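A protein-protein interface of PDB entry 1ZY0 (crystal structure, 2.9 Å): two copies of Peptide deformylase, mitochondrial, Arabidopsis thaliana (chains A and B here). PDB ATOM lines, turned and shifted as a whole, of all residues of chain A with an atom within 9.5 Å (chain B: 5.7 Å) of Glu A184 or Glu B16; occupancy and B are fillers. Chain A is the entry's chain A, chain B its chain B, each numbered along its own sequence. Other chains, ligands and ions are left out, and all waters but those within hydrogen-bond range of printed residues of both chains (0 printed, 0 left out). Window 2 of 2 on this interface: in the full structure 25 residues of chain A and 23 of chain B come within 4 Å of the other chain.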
ATOM      1  N   VAL A 168     -24.573 -16.957 -29.837  1.00  0.00           N
ATOM      2  CA  VAL A 168     -25.942 -17.151 -29.304  1.00  0.00           C
ATOM      3  C   VAL A 168     -25.782 -16.341 -28.107  1.00  0.00           C
ATOM      4  O   VAL A 168     -25.027 -16.290 -27.332  1.00  0.00           O
ATOM      5  CB  VAL A 168     -25.836 -18.582 -29.095  1.00  0.00           C
ATOM      6  CG1 VAL A 168     -26.798 -19.010 -28.064  1.00  0.00           C
ATOM      7  CG2 VAL A 168     -26.079 -19.342 -30.347  1.00  0.00           C
ATOM      8  N   PRO A 169     -27.067 -15.727 -27.832  1.00  0.00           N
ATOM      9  CA  PRO A 169     -27.091 -15.121 -26.589  1.00  0.00           C
ATOM     10  C   PRO A 169     -26.472 -15.703 -25.342  1.00  0.00           C
ATOM     11  O   PRO A 169     -26.755 -16.840 -25.039  1.00  0.00           O
ATOM     12  CB  PRO A 169     -28.474 -14.724 -26.538  1.00  0.00           C
ATOM     13  CG  PRO A 169     -28.828 -14.636 -28.004  1.00  0.00           C
ATOM     14  CD  PRO A 169     -28.254 -15.833 -28.579  1.00  0.00           C
ATOM     15  N   ARG A 170     -25.664 -14.910 -24.642  1.00  0.00           N
ATOM     16  CA  ARG A 170     -25.061 -15.318 -23.385  1.00  0.00           C
ATOM     17  C   ARG A 170     -24.301 -16.624 -23.291  1.00  0.00           C
ATOM     18  O   ARG A 170     -24.502 -17.414 -22.367  1.00  0.00           O
ATOM     19  CB  ARG A 170     -26.096 -15.252 -22.256  1.00  0.00           C
ATOM     20  CG  ARG A 170     -27.475 -15.691 -22.529  1.00  0.00           C
ATOM     21  CD  ARG A 170     -28.473 -14.988 -21.743  1.00  0.00           C
ATOM     22  NE  ARG A 170     -29.834 -15.619 -21.568  1.00  0.00           N
ATOM     23  CZ  ARG A 170     -30.742 -14.773 -21.171  1.00  0.00           C
ATOM     24  NH1 ARG A 170     -31.154 -13.769 -21.756  1.00  0.00           N
ATOM     25  NH2 ARG A 170     -31.767 -15.442 -20.613  1.00  0.00           N
ATOM     26  N   THR A 171     -23.416 -16.830 -24.254  1.00  0.00           N
ATOM     27  CA  THR A 171     -22.545 -17.993 -24.305  1.00  0.00           C
ATOM     28  C   THR A 171     -21.155 -17.364 -24.355  1.00  0.00           C
ATOM     29  O   THR A 171     -20.158 -17.987 -24.025  1.00  0.00           O
ATOM     30  CB  THR A 171     -22.804 -18.859 -25.560  1.00  0.00           C
ATOM     31  OG1 THR A 171     -22.512 -18.109 -26.742  1.00  0.00           O
ATOM     32  CG2 THR A 171     -24.250 -19.302 -25.595  1.00  0.00           C
ATOM     33  N   ARG A 173     -17.855 -15.662 -23.553  1.00  0.00           N
ATOM     34  CA  ARG A 173     -17.132 -15.902 -22.314  1.00  0.00           C
ATOM     35  C   ARG A 173     -15.641 -15.749 -22.385  1.00  0.00           C
ATOM     36  O   ARG A 173     -15.061 -15.597 -23.449  1.00  0.00           O
ATOM     37  CB  ARG A 173     -17.420 -17.306 -21.817  1.00  0.00           C
ATOM     38  CG  ARG A 173     -16.927 -18.380 -22.765  1.00  0.00           C
ATOM     39  CD  ARG A 173     -17.521 -19.722 -22.386  1.00  0.00           C
ATOM     40  NE  ARG A 173     -18.973 -19.627 -22.286  1.00  0.00           N
ATOM     41  CZ  ARG A 173     -19.735 -20.478 -21.617  1.00  0.00           C
ATOM     42  NH1 ARG A 173     -19.187 -21.499 -20.987  1.00  0.00           N
ATOM     43  NH2 ARG A 173     -21.044 -20.295 -21.565  1.00  0.00           N
ATOM     44  N   PRO A 181     -20.409 -24.464 -17.535  1.00  0.00           N
ATOM     45  CA  PRO A 181     -21.735 -24.835 -18.030  1.00  0.00           C
ATOM     46  C   PRO A 181     -22.486 -23.725 -18.736  1.00  0.00           C
ATOM     47  O   PRO A 181     -22.380 -22.555 -18.379  1.00  0.00           O
ATOM     48  CB  PRO A 181     -22.452 -25.275 -16.767  1.00  0.00           C
ATOM     49  CG  PRO A 181     -21.335 -25.816 -15.912  1.00  0.00           C
ATOM     50  CD  PRO A 181     -20.279 -24.771 -16.100  1.00  0.00           C
ATOM     51  N   LEU A 182     -23.255 -24.100 -19.745  1.00  0.00           N
ATOM     52  CA  LEU A 182     -24.054 -23.120 -20.465  1.00  0.00           C
ATOM     53  C   LEU A 182     -25.151 -22.672 -19.517  1.00  0.00           C
ATOM     54  O   LEU A 182     -25.578 -23.433 -18.652  1.00  0.00           O
ATOM     55  CB  LEU A 182     -24.728 -23.738 -21.687  1.00  0.00           C
ATOM     56  CG  LEU A 182     -23.946 -24.256 -22.881  1.00  0.00           C
ATOM     57  CD1 LEU A 182     -24.498 -23.602 -24.092  1.00  0.00           C
ATOM     58  CD2 LEU A 182     -22.511 -23.902 -22.793  1.00  0.00           C
ATOM     59  N   ALA A 183     -25.614 -21.445 -19.678  1.00  0.00           N
ATOM     60  CA  ALA A 183     -26.693 -20.964 -18.837  1.00  0.00           C
ATOM     61  C   ALA A 183     -27.944 -21.669 -19.345  1.00  0.00           C
ATOM     62  O   ALA A 183     -27.991 -22.094 -20.496  1.00  0.00           O
ATOM     63  CB  ALA A 183     -26.831 -19.450 -18.984  1.00  0.00           C
ATOM     64  N   GLU A 184     -28.951 -21.820 -18.495  1.00  0.00           N
ATOM     65  CA  GLU A 184     -30.173 -22.479 -18.935  1.00  0.00           C
ATOM     66  C   GLU A 184     -30.810 -21.606 -20.009  1.00  0.00           C
ATOM     67  O   GLU A 184     -30.724 -20.376 -19.950  1.00  0.00           O
ATOM     68  CB  GLU A 184     -31.123 -22.657 -17.773  1.00  0.00           C
ATOM     69  N   GLY A 185     -31.446 -22.242 -20.992  1.00  0.00           N
ATOM     70  CA  GLY A 185     -32.077 -21.495 -22.072  1.00  0.00           C
ATOM     71  C   GLY A 185     -31.168 -21.384 -23.281  1.00  0.00           C
ATOM     72  O   GLY A 185     -31.558 -20.851 -24.318  1.00  0.00           O
ATOM     73  N   CYS A 186     -29.945 -21.893 -23.142  1.00  0.00           N
ATOM     74  CA  CYS A 186     -28.972 -21.872 -24.217  1.00  0.00           C
ATOM     75  C   CYS A 186     -29.055 -23.143 -25.015  1.00  0.00           C
ATOM     76  O   CYS A 186     -29.089 -24.228 -24.452  1.00  0.00           O
ATOM     77  CB  CYS A 186     -27.571 -21.733 -23.654  1.00  0.00           C
ATOM     78  SG  CYS A 186     -27.208 -20.110 -23.034  1.00  0.00           S
ATOM     79  N   PRO A 187     -29.076 -23.037 -26.351  1.00  0.00           N
ATOM     80  CA  PRO A 187     -29.153 -24.264 -27.138  1.00  0.00           C
ATOM     81  C   PRO A 187     -28.008 -25.135 -26.674  1.00  0.00           C
ATOM     82  O   PRO A 187     -27.030 -24.624 -26.162  1.00  0.00           O
ATOM     83  CB  PRO A 187     -28.943 -23.774 -28.571  1.00  0.00           C
ATOM     84  CG  PRO A 187     -29.390 -22.342 -28.530  1.00  0.00           C
ATOM     85  CD  PRO A 187     -28.836 -21.871 -27.219  1.00  0.00           C
ATOM     86  N   LYS A 188     -28.126 -26.441 -26.822  1.00  0.00           N
ATOM     87  CA  LYS A 188     -27.026 -27.297 -26.420  1.00  0.00           C
ATOM     88  C   LYS A 188     -26.078 -27.430 -27.628  1.00  0.00           C
ATOM     89  O   LYS A 188     -26.513 -27.263 -28.777  1.00  0.00           O
ATOM     90  CB  LYS A 188     -27.552 -28.663 -25.977  1.00  0.00           C
ATOM     91  N   PRO B  12     -22.078 -19.035 -15.247  1.00  0.00           N
ATOM     92  CA  PRO B  12     -23.537 -19.119 -15.231  1.00  0.00           C
ATOM     93  C   PRO B  12     -24.275 -18.045 -14.440  1.00  0.00           C
ATOM     94  O   PRO B  12     -25.329 -17.570 -14.864  1.00  0.00           O
ATOM     95  CB  PRO B  12     -23.779 -20.508 -14.673  1.00  0.00           C
ATOM     96  CG  PRO B  12     -22.669 -21.271 -15.277  1.00  0.00           C
ATOM     97  CD  PRO B  12     -21.491 -20.367 -15.038  1.00  0.00           C
ATOM     98  N   VAL B  13     -23.720 -17.660 -13.299  1.00  0.00           N
ATOM     99  CA  VAL B  13     -24.372 -16.666 -12.468  1.00  0.00           C
ATOM    100  C   VAL B  13     -24.687 -15.400 -13.252  1.00  0.00           C
ATOM    101  O   VAL B  13     -25.739 -14.797 -13.073  1.00  0.00           O
ATOM    102  CB  VAL B  13     -23.512 -16.304 -11.244  1.00  0.00           C
ATOM    103  CG1 VAL B  13     -22.280 -15.558 -11.678  1.00  0.00           C
ATOM    104  CG2 VAL B  13     -24.323 -15.476 -10.271  1.00  0.00           C
ATOM    105  N   LEU B  14     -23.777 -15.010 -14.130  1.00  0.00           N
ATOM    106  CA  LEU B  14     -23.949 -13.814 -14.935  1.00  0.00           C
ATOM    107  C   LEU B  14     -25.029 -13.927 -15.994  1.00  0.00           C
ATOM    108  O   LEU B  14     -25.617 -12.929 -16.375  1.00  0.00           O
ATOM    109  CB  LEU B  14     -22.637 -13.439 -15.619  1.00  0.00           C
ATOM    110  CG  LEU B  14     -21.638 -12.621 -14.826  1.00  0.00           C
ATOM    111  CD1 LEU B  14     -20.408 -12.409 -15.660  1.00  0.00           C
ATOM    112  CD2 LEU B  14     -22.253 -11.302 -14.462  1.00  0.00           C
ATOM    113  N   HIS B  15     -25.290 -15.130 -16.489  1.00  0.00           N
ATOM    114  CA  HIS B  15     -26.285 -15.300 -17.537  1.00  0.00           C
ATOM    115  C   HIS B  15     -27.538 -16.050 -17.114  1.00  0.00           C
ATOM    116  O   HIS B  15     -28.058 -16.865 -17.866  1.00  0.00           O
ATOM    117  CB  HIS B  15     -25.656 -16.006 -18.739  1.00  0.00           C
ATOM    118  CG  HIS B  15     -24.221 -15.645 -18.965  1.00  0.00           C
ATOM    119  ND1 HIS B  15     -23.188 -16.372 -18.432  1.00  0.00           N
ATOM    120  CD2 HIS B  15     -23.656 -14.623 -19.647  1.00  0.00           C
ATOM    121  CE1 HIS B  15     -22.037 -15.817 -18.776  1.00  0.00           C
ATOM    122  NE2 HIS B  15     -22.294 -14.758 -19.514  1.00  0.00           N
ATOM    123  N   GLU B  16     -28.021 -15.774 -15.913  1.00  0.00           N
ATOM    124  CA  GLU B  16     -29.227 -16.417 -15.414  1.00  0.00           C
ATOM    125  C   GLU B  16     -29.956 -15.404 -14.541  1.00  0.00           C
ATOM    126  O   GLU B  16     -29.317 -14.601 -13.861  1.00  0.00           O
ATOM    127  CB  GLU B  16     -28.890 -17.651 -14.579  1.00  0.00           C
ATOM    128  CG  GLU B  16     -28.103 -18.740 -15.293  1.00  0.00           C
ATOM    129  CD  GLU B  16     -27.819 -19.933 -14.394  1.00  0.00           C
ATOM    130  OE1 GLU B  16     -27.315 -19.735 -13.262  1.00  0.00           O
ATOM    131  OE2 GLU B  16     -28.101 -21.069 -14.830  1.00  0.00           O
ATOM    132  N   LYS B  17     -31.288 -15.443 -14.551  1.00  0.00           N
ATOM    133  CA  LYS B  17     -32.084 -14.512 -13.764  1.00  0.00           C
ATOM    134  C   LYS B  17     -31.821 -14.649 -12.271  1.00  0.00           C
ATOM    135  O   LYS B  17     -31.872 -15.747 -11.724  1.00  0.00           O
ATOM    136  CB  LYS B  17     -33.563 -14.708 -14.064  1.00  0.00           C
ATOM    137  N   ALA B  18     -31.512 -13.514 -11.621  1.00  0.00           N
ATOM    138  CA  ALA B  18     -31.245 -13.512 -10.191  1.00  0.00           C
ATOM    139  C   ALA B  18     -32.561 -13.445  -9.445  1.00  0.00           C
ATOM    140  O   ALA B  18     -33.527 -12.874  -9.938  1.00  0.00           O
ATOM    141  CB  ALA B  18     -30.388 -12.337  -9.826  1.00  0.00           C
ATOM    142  N   PRO B  53     -25.030 -10.378  -9.033  1.00  0.00           N
ATOM    143  CA  PRO B  53     -24.460 -11.491  -9.782  1.00  0.00           C
ATOM    144  C   PRO B  53     -23.003 -11.283 -10.175  1.00  0.00           C
ATOM    145  O   PRO B  53     -22.258 -12.246 -10.320  1.00  0.00           O
ATOM    146  CB  PRO B  53     -25.384 -11.590 -10.990  1.00  0.00           C
ATOM    147  CG  PRO B  53     -26.693 -11.134 -10.441  1.00  0.00           C
ATOM    148  CD  PRO B  53     -26.276  -9.920  -9.670  1.00  0.00           C
ATOM    149  N   HIS B 157     -28.023  -7.140 -16.032  1.00  0.00           N
ATOM    150  CA  HIS B 157     -27.202  -8.118 -15.345  1.00  0.00           C
ATOM    151  C   HIS B 157     -28.088  -9.011 -14.517  1.00  0.00           C
ATOM    152  O   HIS B 157     -27.855 -10.208 -14.421  1.00  0.00           O
ATOM    153  CB  HIS B 157     -26.205  -7.434 -14.413  1.00  0.00           C
ATOM    154  CG  HIS B 157     -24.953  -6.982 -15.091  1.00  0.00           C
ATOM    155  ND1 HIS B 157     -24.032  -7.854 -15.613  1.00  0.00           N
ATOM    156  CD2 HIS B 157     -24.469  -5.746 -15.326  1.00  0.00           C
ATOM    157  CE1 HIS B 157     -23.033  -7.177 -16.145  1.00  0.00           C
ATOM    158  NE2 HIS B 157     -23.279  -5.895 -15.982  1.00  0.00           N
ATOM    159  N   LEU B 158     -29.115  -8.417 -13.926  1.00  0.00           N
ATOM    160  CA  LEU B 158     -30.035  -9.160 -13.081  1.00  0.00           C
ATOM    161  C   LEU B 158     -30.932 -10.125 -13.850  1.00  0.00           C
ATOM    162  O   LEU B 158     -31.648 -10.919 -13.247  1.00  0.00           O
ATOM    163  CB  LEU B 158     -30.891  -8.195 -12.264  1.00  0.00           C
ATOM    164  CG  LEU B 158     -30.143  -7.264 -11.303  1.00  0.00           C
ATOM    165  CD1 LEU B 158     -31.151  -6.460 -10.493  1.00  0.00           C
ATOM    166  CD2 LEU B 158     -29.247  -8.073 -10.379  1.00  0.00           C
ATOM    167  N   ASP B 159     -30.903 -10.063 -15.175  1.00  0.00           N
ATOM    168  CA  ASP B 159     -31.726 -10.966 -15.961  1.00  0.00           C
ATOM    169  C   ASP B 159     -30.890 -11.907 -16.796  1.00  0.00           C
ATOM    170  O   ASP B 159     -31.434 -12.688 -17.573  1.00  0.00           O
ATOM    171  CB  ASP B 159     -32.682 -10.197 -16.865  1.00  0.00           C
ATOM    172  CG  ASP B 159     -33.912  -9.705 -16.127  1.00  0.00           C
ATOM    173  OD1 ASP B 159     -34.626 -10.540 -15.547  1.00  0.00           O
ATOM    174  OD2 ASP B 159     -34.166  -8.480 -16.129  1.00  0.00           O
ATOM    175  N   GLY B 160     -29.572 -11.834 -16.630  1.00  0.00           N
ATOM    176  CA  GLY B 160     -28.668 -12.694 -17.375  1.00  0.00           C
ATOM    177  C   GLY B 160     -28.260 -12.112 -18.711  1.00  0.00           C
ATOM    178  O   GLY B 160     -27.656 -12.789 -19.547  1.00  0.00           O
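O of Ala A183 sits close to SG of Cys A186 (3.3 Å).
Among the printed residues, pairs that only touch across the chains: Arg A170 with His B15, Arg A170 with Gly B160, Pro A181 with Pro B12, Ala A183 with His B15, Ala A183 with Glu B16 and Glu A184 with Glu B16.
Of the printed residues of chain B, Glu A184 touches Glu B16.
Glu B16 touches two residues of chain A.
No residue of chain A comes within 4 Å of Lys B17.
Of the printed residues of chain A, Gly B160 touches Arg A170.
Of the printed residues of chain A, His B15 touches Arg A170 (3.6 Å) and Ala A183 (3.1 Å).
Of the printed residues of chain A, Pro B12 touches Pro A181.
Gly A185 touches none of the printed residues of chain B.
Leu B158 touches none of the printed residues of chain A.
The nearest printed residue of chain B that does not touch Arg A170 is Asp B159 (4.1 Å).
Printed residues of chain A that touch a printed residue of chain B: Arg A170, Pro A181, Ala A183 and Glu A184.
Hydrophobic or aromatic side chains of chain A that line the printed part of chain B: Ala A183.
Of the 12 printed residues of chain B, 4 touch a printed residue of chain A.
Printed residues of chain B that touch a printed residue of chain A: Pro B12, His B15, Glu B16 and Gly B160.
Among the printed residues, no Asp or Glu carboxylate lies within 4 Å of a Lys or Arg side-chain nitrogen of the other chain.
No position is printed for both chains.
Of the 6 pairs that touch across the chains among the printed residues, none has its exchanged pair printed and touching as well.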
